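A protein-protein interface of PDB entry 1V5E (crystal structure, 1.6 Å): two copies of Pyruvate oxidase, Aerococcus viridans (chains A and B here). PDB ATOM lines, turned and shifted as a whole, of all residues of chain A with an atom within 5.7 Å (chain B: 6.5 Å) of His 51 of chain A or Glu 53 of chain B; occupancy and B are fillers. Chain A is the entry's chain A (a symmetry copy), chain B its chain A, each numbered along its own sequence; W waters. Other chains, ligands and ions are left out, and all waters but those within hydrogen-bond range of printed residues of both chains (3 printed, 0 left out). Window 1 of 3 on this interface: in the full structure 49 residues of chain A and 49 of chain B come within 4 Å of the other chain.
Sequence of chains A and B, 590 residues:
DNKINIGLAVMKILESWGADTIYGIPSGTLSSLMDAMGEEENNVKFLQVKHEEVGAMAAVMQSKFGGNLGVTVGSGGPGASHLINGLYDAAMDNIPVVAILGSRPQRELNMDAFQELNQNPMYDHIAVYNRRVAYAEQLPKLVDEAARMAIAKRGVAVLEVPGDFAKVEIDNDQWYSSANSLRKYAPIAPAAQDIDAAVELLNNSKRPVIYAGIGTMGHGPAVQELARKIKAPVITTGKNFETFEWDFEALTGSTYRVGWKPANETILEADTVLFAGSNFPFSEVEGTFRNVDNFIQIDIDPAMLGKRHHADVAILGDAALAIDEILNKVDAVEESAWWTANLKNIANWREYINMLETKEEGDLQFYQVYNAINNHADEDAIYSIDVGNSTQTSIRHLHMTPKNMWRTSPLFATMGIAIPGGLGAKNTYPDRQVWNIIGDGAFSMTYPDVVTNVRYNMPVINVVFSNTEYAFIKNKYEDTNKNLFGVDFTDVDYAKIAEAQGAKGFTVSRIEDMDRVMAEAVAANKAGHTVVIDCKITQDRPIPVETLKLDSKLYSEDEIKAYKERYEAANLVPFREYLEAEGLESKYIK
Of the 11 printed residues of chain A, 6 touch a printed residue of chain B. Along chain A the printed residues that touch a printed residue of chain B span positions 25 to 82.
His 51 of chain A touches Glu 53 of chain B, and with the chains exchanged Glu 53 of chain A touches His 51 of chain B. Glu 53 of chain A touches His 82 of chain B, and with the chains exchanged His 82 of chain A touches Glu 53 of chain B. 8 positions are printed for both chains. Of the 11 pairs that touch across the chains among the printed residues, 4 have their exchanged pair printed and touching as well.
OE2 of Glu 53 of chain A is in hydrogen-bond range of NE2 of His 51 of chain B, 2.8 Å away. The side-chain carboxylate of Glu 53 of chain B sits at hydrogen-bond distance from a ring nitrogen (NE2) of His 51 of chain A (2.8 Å). OE1 of Glu 53 of chain B is in hydrogen-bond range of NE2 of His 82 of chain A, 2.7 Å away. NE2 of His 82 of chain B sits at hydrogen-bond distance from OE1 of Glu 53 of chain A (2.7 Å). ND2 of Asn 85 of chain B is in hydrogen-bond range of NE2 of His 82 of chain A (3.3 Å).
Glu 53 of chain B touches two residues of chain A. Of the printed residues of chain A, His 51 of chain B touches Glu 53 (2.8 Å). Of the printed residues of chain B, Ile 25 of chain A touches Met 445. The nearest residue of chain A that does not touch Glu 53 of chain B is Glu 53 of chain A (5.5 Å).
Water W2 lies within hydrogen-bond range of the side-chain carboxylate of Glu 52 of chain A (2.8 Å) and the side-chain sulfur of Met 415 of chain B (3.5 Å). Water W1 lies within hydrogen-bond range of O of Met 415 of chain B (2.9 Å), OE2 of Glu 53 of chain B (3.1 Å) and NE2 of His 82 of chain A (3.4 Å). Water W3 lies within hydrogen-bond range of the side-chain carboxylate (OE2) of Glu 53 of chain A and a ring nitrogen (NE2) of His 82 of chain B.
A ring nitrogen (ND1) of His 51 of chain B sits close to the backbone NH (N) of Glu 53 of chain B (3.1 Å). N of Glu 53 of chain B lies close to O of His 82 of chain B (3.5 Å). ND2 of Asn 85 of chain B is in hydrogen-bond range of OG1 of Thr 414 of chain B. NE2 of His 82 of chain A sits at hydrogen-bond distance from NE2 of His 51 of chain A (3.3 Å). OE1 of Glu 52 of chain A sits at hydrogen-bond distance from ND1 of His 82 of chain A (2.8 Å). N of Glu 53 of chain A lies close to O of His 82 of chain A (3.5 Å).
Among the printed residues, merely in contact across the chains: Lys 50 of chain A with Met 445 of chain B (3.2 Å), Lys 50 of chain A with Ser 444 of chain B (3.5 Å), Ile 25 of chain A with Met 445 of chain B (3.6 Å), Glu 52 of chain A with Met 445 of chain B (3.6 Å), His 51 of chain A with Met 445 of chain B (3.8 Å) and His 82 of chain A with Met 445 of chain B (3.9 Å).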
ATOM      1  N   ILE A  25      19.764  31.870  -8.630  1.00  0.00           N
ATOM      2  CA  ILE A  25      20.589  31.359  -9.713  1.00  0.00           C
ATOM      3  C   ILE A  25      19.682  31.137 -10.917  1.00  0.00           C
ATOM      4  O   ILE A  25      18.612  30.544 -10.793  1.00  0.00           O
ATOM      5  CB  ILE A  25      21.254  30.023  -9.318  1.00  0.00           C
ATOM      6  CG1 ILE A  25      22.144  30.236  -8.089  1.00  0.00           C
ATOM      7  CG2 ILE A  25      22.078  29.485 -10.473  1.00  0.00           C
ATOM      8  CD1 ILE A  25      22.831  28.983  -7.592  1.00  0.00           C
ATOM      9  N   VAL A  49      23.876  34.291  -6.910  1.00  0.00           N
ATOM     10  CA  VAL A  49      24.730  33.681  -5.895  1.00  0.00           C
ATOM     11  C   VAL A  49      25.293  32.356  -6.404  1.00  0.00           C
ATOM     12  O   VAL A  49      24.953  31.911  -7.501  1.00  0.00           O
ATOM     13  CB  VAL A  49      23.941  33.427  -4.595  1.00  0.00           C
ATOM     14  CG1 VAL A  49      23.511  34.755  -3.983  1.00  0.00           C
ATOM     15  CG2 VAL A  49      22.721  32.563  -4.890  1.00  0.00           C
ATOM     16  N   LYS A  50      26.153  31.726  -5.611  1.00  0.00           N
ATOM     17  CA  LYS A  50      26.744  30.453  -6.010  1.00  0.00           C
ATOM     18  C   LYS A  50      25.938  29.262  -5.499  1.00  0.00           C
ATOM     19  O   LYS A  50      25.972  28.186  -6.088  1.00  0.00           O
ATOM     20  CB  LYS A  50      28.186  30.339  -5.505  1.00  0.00           C
ATOM     21  CG  LYS A  50      29.118  31.445  -5.985  1.00  0.00           C
ATOM     22  CD  LYS A  50      28.976  31.708  -7.482  1.00  0.00           C
ATOM     23  CE  LYS A  50      29.254  30.472  -8.319  1.00  0.00           C
ATOM     24  NZ  LYS A  50      29.092  30.771  -9.770  1.00  0.00           N
ATOM     25  N   HIS A  51      25.217  29.461  -4.399  1.00  0.00           N
ATOM     26  CA  HIS A  51      24.393  28.406  -3.816  1.00  0.00           C
ATOM     27  C   HIS A  51      23.074  29.069  -3.430  1.00  0.00           C
ATOM     28  O   HIS A  51      23.069  30.096  -2.753  1.00  0.00           O
ATOM     29  CB  HIS A  51      25.093  27.825  -2.581  1.00  0.00           C
ATOM     30  CG  HIS A  51      24.484  26.554  -2.078  1.00  0.00           C
ATOM     31  ND1 HIS A  51      23.212  26.494  -1.549  1.00  0.00           N
ATOM     32  CD2 HIS A  51      24.977  25.295  -2.014  1.00  0.00           C
ATOM     33  CE1 HIS A  51      22.950  25.253  -1.181  1.00  0.00           C
ATOM     34  NE2 HIS A  51      24.004  24.505  -1.453  1.00  0.00           N
ATOM     35  N   GLU A  52      21.957  28.490  -3.864  1.00  0.00           N
ATOM     36  CA  GLU A  52      20.658  29.097  -3.582  1.00  0.00           C
ATOM     37  C   GLU A  52      20.364  29.368  -2.116  1.00  0.00           C
ATOM     38  O   GLU A  52      19.595  30.277  -1.799  1.00  0.00           O
ATOM     39  CB  GLU A  52      19.524  28.262  -4.188  1.00  0.00           C
ATOM     40  CG  GLU A  52      19.590  28.148  -5.700  1.00  0.00           C
ATOM     41  CD  GLU A  52      20.283  26.883  -6.151  1.00  0.00           C
ATOM     42  OE1 GLU A  52      21.092  26.332  -5.373  1.00  0.00           O
ATOM     43  OE2 GLU A  52      20.021  26.446  -7.289  1.00  0.00           O
ATOM     44  N   GLU A  53      20.969  28.607  -1.210  1.00  0.00           N
ATOM     45  CA  GLU A  53      20.698  28.848   0.199  1.00  0.00           C
ATOM     46  C   GLU A  53      21.232  30.223   0.596  1.00  0.00           C
ATOM     47  O   GLU A  53      20.647  30.905   1.437  1.00  0.00           O
ATOM     48  CB  GLU A  53      21.292  27.740   1.082  1.00  0.00           C
ATOM     49  CG  GLU A  53      22.739  27.889   1.493  1.00  0.00           C
ATOM     50  CD  GLU A  53      23.131  26.828   2.502  1.00  0.00           C
ATOM     51  OE1 GLU A  53      22.342  26.599   3.444  1.00  0.00           O
ATOM     52  OE2 GLU A  53      24.214  26.227   2.364  1.00  0.00           O
ATOM     53  N   VAL A  54      22.331  30.642  -0.024  1.00  0.00           N
ATOM     54  CA  VAL A  54      22.893  31.954   0.266  1.00  0.00           C
ATOM     55  C   VAL A  54      21.950  33.030  -0.286  1.00  0.00           C
ATOM     56  O   VAL A  54      21.818  34.108   0.297  1.00  0.00           O
ATOM     57  CB  VAL A  54      24.312  32.106  -0.343  1.00  0.00           C
ATOM     58  CG1 VAL A  54      24.773  33.558  -0.262  1.00  0.00           C
ATOM     59  CG2 VAL A  54      25.287  31.216   0.423  1.00  0.00           C
ATOM     60  N   GLY A  55      21.287  32.730  -1.400  1.00  0.00           N
ATOM     61  CA  GLY A  55      20.348  33.681  -1.969  1.00  0.00           C
ATOM     62  C   GLY A  55      19.153  33.842  -1.045  1.00  0.00           C
ATOM     63  O   GLY A  55      18.677  34.955  -0.809  1.00  0.00           O
ATOM     64  N   ALA A  56      18.661  32.727  -0.512  1.00  0.00           N
ATOM     65  CA  ALA A  56      17.523  32.777   0.399  1.00  0.00           C
ATOM     66  C   ALA A  56      17.888  33.528   1.680  1.00  0.00           C
ATOM     67  O   ALA A  56      17.150  34.408   2.128  1.00  0.00           O
ATOM     68  CB  ALA A  56      17.049  31.359   0.733  1.00  0.00           C
ATOM     69  N   HIS A  82      17.024  23.949  -1.983  1.00  0.00           N
ATOM     70  CA  HIS A  82      18.223  24.584  -1.447  1.00  0.00           C
ATOM     71  C   HIS A  82      17.911  25.834  -0.623  1.00  0.00           C
ATOM     72  O   HIS A  82      18.757  26.311   0.127  1.00  0.00           O
ATOM     73  CB  HIS A  82      19.178  24.949  -2.584  1.00  0.00           C
ATOM     74  CG  HIS A  82      20.301  23.978  -2.763  1.00  0.00           C
ATOM     75  ND1 HIS A  82      21.174  24.042  -3.827  1.00  0.00           N
ATOM     76  CD2 HIS A  82      20.711  22.937  -2.001  1.00  0.00           C
ATOM     77  CE1 HIS A  82      22.072  23.080  -3.715  1.00  0.00           C
ATOM     78  NE2 HIS A  82      21.813  22.395  -2.615  1.00  0.00           N
ATOM     79  N   ASP A 449      30.741  31.660  -1.928  1.00  0.00           N
ATOM     80  CA  ASP A 449      30.003  32.879  -2.240  1.00  0.00           C
ATOM     81  C   ASP A 449      30.748  34.175  -1.939  1.00  0.00           C
ATOM     82  O   ASP A 449      30.192  35.269  -2.052  1.00  0.00           O
ATOM     83  CB  ASP A 449      28.624  32.848  -1.570  1.00  0.00           C
ATOM     84  CG  ASP A 449      27.543  32.343  -2.514  1.00  0.00           C
ATOM     85  OD1 ASP A 449      27.180  33.094  -3.444  1.00  0.00           O
ATOM     86  OD2 ASP A 449      27.065  31.196  -2.349  1.00  0.00           O
ATOM     87  N   VAL B  49      31.933  15.660   6.932  1.00  0.00           N
ATOM     88  CA  VAL B  49      31.922  16.502   5.740  1.00  0.00           C
ATOM     89  C   VAL B  49      31.901  17.977   6.135  1.00  0.00           C
ATOM     90  O   VAL B  49      31.826  18.308   7.319  1.00  0.00           O
ATOM     91  CB  VAL B  49      30.690  16.198   4.865  1.00  0.00           C
ATOM     92  CG1 VAL B  49      30.778  14.775   4.325  1.00  0.00           C
ATOM     93  CG2 VAL B  49      29.417  16.373   5.684  1.00  0.00           C
ATOM     94  N   HIS B  51      29.661  20.233   4.617  1.00  0.00           N
ATOM     95  CA  HIS B  51      28.276  20.677   4.498  1.00  0.00           C
ATOM     96  C   HIS B  51      27.423  19.413   4.569  1.00  0.00           C
ATOM     97  O   HIS B  51      27.671  18.454   3.840  1.00  0.00           O
ATOM     98  CB  HIS B  51      28.075  21.395   3.158  1.00  0.00           C
ATOM     99  CG  HIS B  51      26.782  22.140   3.054  1.00  0.00           C
ATOM    100  ND1 HIS B  51      25.556  21.510   3.050  1.00  0.00           N
ATOM    101  CD2 HIS B  51      26.524  23.465   2.942  1.00  0.00           C
ATOM    102  CE1 HIS B  51      24.599  22.414   2.938  1.00  0.00           C
ATOM    103  NE2 HIS B  51      25.160  23.609   2.871  1.00  0.00           N
ATOM    104  N   GLU B  52      26.423  19.407   5.447  1.00  0.00           N
ATOM    105  CA  GLU B  52      25.598  18.213   5.611  1.00  0.00           C
ATOM    106  C   GLU B  52      24.950  17.682   4.343  1.00  0.00           C
ATOM    107  O   GLU B  52      24.676  16.485   4.246  1.00  0.00           O
ATOM    108  CB  GLU B  52      24.523  18.437   6.681  1.00  0.00           C
ATOM    109  CG  GLU B  52      25.085  18.725   8.062  1.00  0.00           C
ATOM    110  CD  GLU B  52      25.174  20.207   8.348  1.00  0.00           C
ATOM    111  OE1 GLU B  52      25.246  21.001   7.385  1.00  0.00           O
ATOM    112  OE2 GLU B  52      25.180  20.573   9.540  1.00  0.00           O
ATOM    113  N   GLU B  53      24.710  18.544   3.360  1.00  0.00           N
ATOM    114  CA  GLU B  53      24.088  18.056   2.139  1.00  0.00           C
ATOM    115  C   GLU B  53      25.036  17.090   1.430  1.00  0.00           C
ATOM    116  O   GLU B  53      24.599  16.127   0.805  1.00  0.00           O
ATOM    117  CB  GLU B  53      23.676  19.214   1.217  1.00  0.00           C
ATOM    118  CG  GLU B  53      24.732  19.757   0.281  1.00  0.00           C
ATOM    119  CD  GLU B  53      24.138  20.762  -0.686  1.00  0.00           C
ATOM    120  OE1 GLU B  53      23.053  20.474  -1.233  1.00  0.00           O
ATOM    121  OE2 GLU B  53      24.743  21.830  -0.903  1.00  0.00           O
ATOM    122  N   VAL B  54      26.338  17.336   1.546  1.00  0.00           N
ATOM    123  CA  VAL B  54      27.318  16.449   0.932  1.00  0.00           C
ATOM    124  C   VAL B  54      27.316  15.112   1.682  1.00  0.00           C
ATOM    125  O   VAL B  54      27.526  14.056   1.084  1.00  0.00           O
ATOM    126  CB  VAL B  54      28.735  17.081   0.945  1.00  0.00           C
ATOM    127  CG1 VAL B  54      29.783  16.047   0.548  1.00  0.00           C
ATOM    128  CG2 VAL B  54      28.774  18.251  -0.034  1.00  0.00           C
ATOM    129  N   GLY B  55      27.065  15.160   2.989  1.00  0.00           N
ATOM    130  CA  GLY B  55      27.011  13.934   3.767  1.00  0.00           C
ATOM    131  C   GLY B  55      25.806  13.109   3.347  1.00  0.00           C
ATOM    132  O   GLY B  55      25.893  11.889   3.192  1.00  0.00           O
ATOM    133  N   ALA B  56      24.669  13.775   3.156  1.00  0.00           N
ATOM    134  CA  ALA B  56      23.459  13.075   2.738  1.00  0.00           C
ATOM    135  C   ALA B  56      23.636  12.474   1.344  1.00  0.00           C
ATOM    136  O   ALA B  56      23.323  11.304   1.116  1.00  0.00           O
ATOM    137  CB  ALA B  56      22.263  14.032   2.755  1.00  0.00           C
ATOM    138  N   MET B  57      24.144  13.273   0.410  1.00  0.00           N
ATOM    139  CA  MET B  57      24.349  12.788  -0.946  1.00  0.00           C
ATOM    140  C   MET B  57      25.368  11.656  -0.992  1.00  0.00           C
ATOM    141  O   MET B  57      25.221  10.719  -1.773  1.00  0.00           O
ATOM    142  CB  MET B  57      24.799  13.929  -1.860  1.00  0.00           C
ATOM    143  CG  MET B  57      23.710  14.939  -2.149  1.00  0.00           C
ATOM    144  SD  MET B  57      24.247  16.181  -3.338  1.00  0.00           S
ATOM    145  CE  MET B  57      25.012  17.339  -2.279  1.00  0.00           C
ATOM    146  N   ALA B  58      26.398  11.741  -0.155  1.00  0.00           N
ATOM    147  CA  ALA B  58      27.426  10.710  -0.120  1.00  0.00           C
ATOM    148  C   ALA B  58      26.847   9.389   0.382  1.00  0.00           C
ATOM    149  O   ALA B  58      27.153   8.326  -0.157  1.00  0.00           O
ATOM    150  CB  ALA B  58      28.590  11.156   0.768  1.00  0.00           C
ATOM    151  N   THR B  72      23.149   9.035   7.198  1.00  0.00           N
ATOM    152  CA  THR B  72      23.528  10.438   7.198  1.00  0.00           C
ATOM    153  C   THR B  72      22.866  11.084   8.400  1.00  0.00           C
ATOM    154  O   THR B  72      21.735  10.741   8.753  1.00  0.00           O
ATOM    155  CB  THR B  72      23.082  11.146   5.896  1.00  0.00           C
ATOM    156  OG1 THR B  72      23.370  12.547   5.983  1.00  0.00           O
ATOM    157  CG2 THR B  72      21.591  10.949   5.655  1.00  0.00           C
ATOM    158  N   GLY B  79      21.056  21.528  10.501  1.00  0.00           N
ATOM    159  CA  GLY B  79      21.809  20.374  10.041  1.00  0.00           C
ATOM    160  C   GLY B  79      20.858  19.427   9.337  1.00  0.00           C
ATOM    161  O   GLY B  79      21.136  18.924   8.247  1.00  0.00           O
ATOM    162  N   HIS B  82      19.606  20.701   6.034  1.00  0.00           N
ATOM    163  CA  HIS B  82      20.659  20.689   5.025  1.00  0.00           C
ATOM    164  C   HIS B  82      20.722  19.369   4.254  1.00  0.00           C
ATOM    165  O   HIS B  82      21.340  19.297   3.196  1.00  0.00           O
ATOM    166  CB  HIS B  82      22.015  20.962   5.677  1.00  0.00           C
ATOM    167  CG  HIS B  82      22.485  22.373   5.521  1.00  0.00           C
ATOM    168  ND1 HIS B  82      23.601  22.859   6.167  1.00  0.00           N
ATOM    169  CD2 HIS B  82      22.007  23.395   4.774  1.00  0.00           C
ATOM    170  CE1 HIS B  82      23.789  24.121   5.827  1.00  0.00           C
ATOM    171  NE2 HIS B  82      22.836  24.471   4.982  1.00  0.00           N
ATOM    172  N   LEU B  83      20.076  18.331   4.774  1.00  0.00           N
ATOM    173  CA  LEU B  83      20.085  17.023   4.117  1.00  0.00           C
ATOM    174  C   LEU B  83      19.129  16.927   2.937  1.00  0.00           C
ATOM    175  O   LEU B  83      19.248  16.021   2.106  1.00  0.00           O
ATOM    176  CB  LEU B  83      19.683  15.931   5.112  1.00  0.00           C
ATOM    177  CG  LEU B  83      20.359  15.856   6.477  1.00  0.00           C
ATOM    178  CD1 LEU B  83      19.738  14.711   7.268  1.00  0.00           C
ATOM    179  CD2 LEU B  83      21.863  15.658   6.308  1.00  0.00           C
ATOM    180  N   ILE B  84      18.194  17.868   2.861  1.00  0.00           N
ATOM    181  CA  ILE B  84      17.145  17.830   1.848  1.00  0.00           C
ATOM    182  C   ILE B  84      17.465  17.430   0.409  1.00  0.00           C
ATOM    183  O   ILE B  84      16.806  16.541  -0.129  1.00  0.00           O
ATOM    184  CB  ILE B  84      16.318  19.147   1.850  1.00  0.00           C
ATOM    185  CG1 ILE B  84      15.010  18.924   1.086  1.00  0.00           C
ATOM    186  CG2 ILE B  84      17.112  20.287   1.218  1.00  0.00           C
ATOM    187  CD1 ILE B  84      13.938  19.949   1.404  1.00  0.00           C
ATOM    188  N   ASN B  85      18.458  18.049  -0.224  1.00  0.00           N
ATOM    189  CA  ASN B  85      18.756  17.682  -1.608  1.00  0.00           C
ATOM    190  C   ASN B  85      19.202  16.236  -1.754  1.00  0.00           C
ATOM    191  O   ASN B  85      18.881  15.582  -2.741  1.00  0.00           O
ATOM    192  CB  ASN B  85      19.801  18.625  -2.208  1.00  0.00           C
ATOM    193  CG  ASN B  85      19.207  19.961  -2.589  1.00  0.00           C
ATOM    194  OD1 ASN B  85      18.518  20.591  -1.787  1.00  0.00           O
ATOM    195  ND2 ASN B  85      19.464  20.404  -3.816  1.00  0.00           N
ATOM    196  N   GLY B  86      19.930  15.732  -0.765  1.00  0.00           N
ATOM    197  CA  GLY B  86      20.373  14.351  -0.831  1.00  0.00           C
ATOM    198  C   GLY B  86      19.217  13.388  -0.637  1.00  0.00           C
ATOM    199  O   GLY B  86      19.145  12.344  -1.287  1.00  0.00           O
ATOM    200  N   THR B 414      19.966  17.134  -8.661  1.00  0.00           N
ATOM    201  CA  THR B 414      20.543  18.139  -7.789  1.00  0.00           C
ATOM    202  C   THR B 414      21.995  18.406  -8.181  1.00  0.00           C
ATOM    203  O   THR B 414      22.766  17.478  -8.422  1.00  0.00           O
ATOM    204  CB  THR B 414      20.486  17.704  -6.306  1.00  0.00           C
ATOM    205  OG1 THR B 414      21.040  18.743  -5.488  1.00  0.00           O
ATOM    206  CG2 THR B 414      21.256  16.404  -6.087  1.00  0.00           C
ATOM    207  N   MET B 415      22.353  19.681  -8.278  1.00  0.00           N
ATOM    208  CA  MET B 415      23.721  20.051  -8.616  1.00  0.00           C
ATOM    209  C   MET B 415      24.588  19.768  -7.395  1.00  0.00           C
ATOM    210  O   MET B 415      24.112  19.843  -6.258  1.00  0.00           O
ATOM    211  CB  MET B 415      23.800  21.536  -8.977  1.00  0.00           C
ATOM    212  CG  MET B 415      23.155  21.887 -10.308  1.00  0.00           C
ATOM    213  SD  MET B 415      23.145  23.667 -10.620  1.00  0.00           S
ATOM    214  CE  MET B 415      24.861  23.945 -11.055  1.00  0.00           C
ATOM    215  N   GLY B 416      25.852  19.439  -7.633  1.00  0.00           N
ATOM    216  CA  GLY B 416      26.764  19.154  -6.540  1.00  0.00           C
ATOM    217  C   GLY B 416      26.788  17.697  -6.108  1.00  0.00           C
ATOM    218  O   GLY B 416      27.335  17.365  -5.058  1.00  0.00           O
ATOM    219  N   PRO B 420      30.083  14.370  -3.647  1.00  0.00           N
ATOM    220  CA  PRO B 420      29.574  13.394  -2.677  1.00  0.00           C
ATOM    221  C   PRO B 420      29.631  11.980  -3.271  1.00  0.00           C
ATOM    222  O   PRO B 420      29.932  11.011  -2.574  1.00  0.00           O
ATOM    223  CB  PRO B 420      28.138  13.855  -2.441  1.00  0.00           C
ATOM    224  CG  PRO B 420      28.213  15.325  -2.652  1.00  0.00           C
ATOM    225  CD  PRO B 420      29.131  15.477  -3.840  1.00  0.00           C
ATOM    226  N   SER B 444      31.046  24.939  -7.693  1.00  0.00           N
ATOM    227  CA  SER B 444      30.942  26.079  -6.790  1.00  0.00           C
ATOM    228  C   SER B 444      29.987  25.861  -5.624  1.00  0.00           C
ATOM    229  O   SER B 444      30.032  26.595  -4.637  1.00  0.00           O
ATOM    230  CB  SER B 444      30.531  27.329  -7.568  1.00  0.00           C
ATOM    231  OG  SER B 444      31.558  27.712  -8.467  1.00  0.00           O
ATOM    232  N   MET B 445      29.127  24.855  -5.733  1.00  0.00           N
ATOM    233  CA  MET B 445      28.189  24.563  -4.653  1.00  0.00           C
ATOM    234  C   MET B 445      28.768  23.538  -3.689  1.00  0.00           C
ATOM    235  O   MET B 445      28.245  23.348  -2.592  1.00  0.00           O
ATOM    236  CB  MET B 445      26.876  24.009  -5.209  1.00  0.00           C
ATOM    237  CG  MET B 445      26.114  24.960  -6.101  1.00  0.00           C
ATOM    238  SD  MET B 445      24.526  24.232  -6.544  1.00  0.00           S
ATOM    239  CE  MET B 445      23.836  25.501  -7.614  1.00  0.00           C
ATOM    240  N   THR B 446      29.864  22.895  -4.087  1.00  0.00           N
ATOM    241  CA  THR B 446      30.442  21.845  -3.259  1.00  0.00           C
ATOM    242  C   THR B 446      31.960  21.773  -3.114  1.00  0.00           C
ATOM    243  O   THR B 446      32.450  20.900  -2.400  1.00  0.00           O
ATOM    244  CB  THR B 446      29.994  20.471  -3.780  1.00  0.00           C
ATOM    245  OG1 THR B 446      30.277  20.388  -5.185  1.00  0.00           O
ATOM    246  CG2 THR B 446      28.504  20.273  -3.565  1.00  0.00           C
HETATM  247  O   HOH W   1      24.763  21.374  -3.943  1.00  0.00           O
HETATM  248  O   HOH W   2      20.653  23.874  -8.122  1.00  0.00           O
HETATM  249  O   HOH W   3      25.144  26.946   5.205  1.00  0.00           O
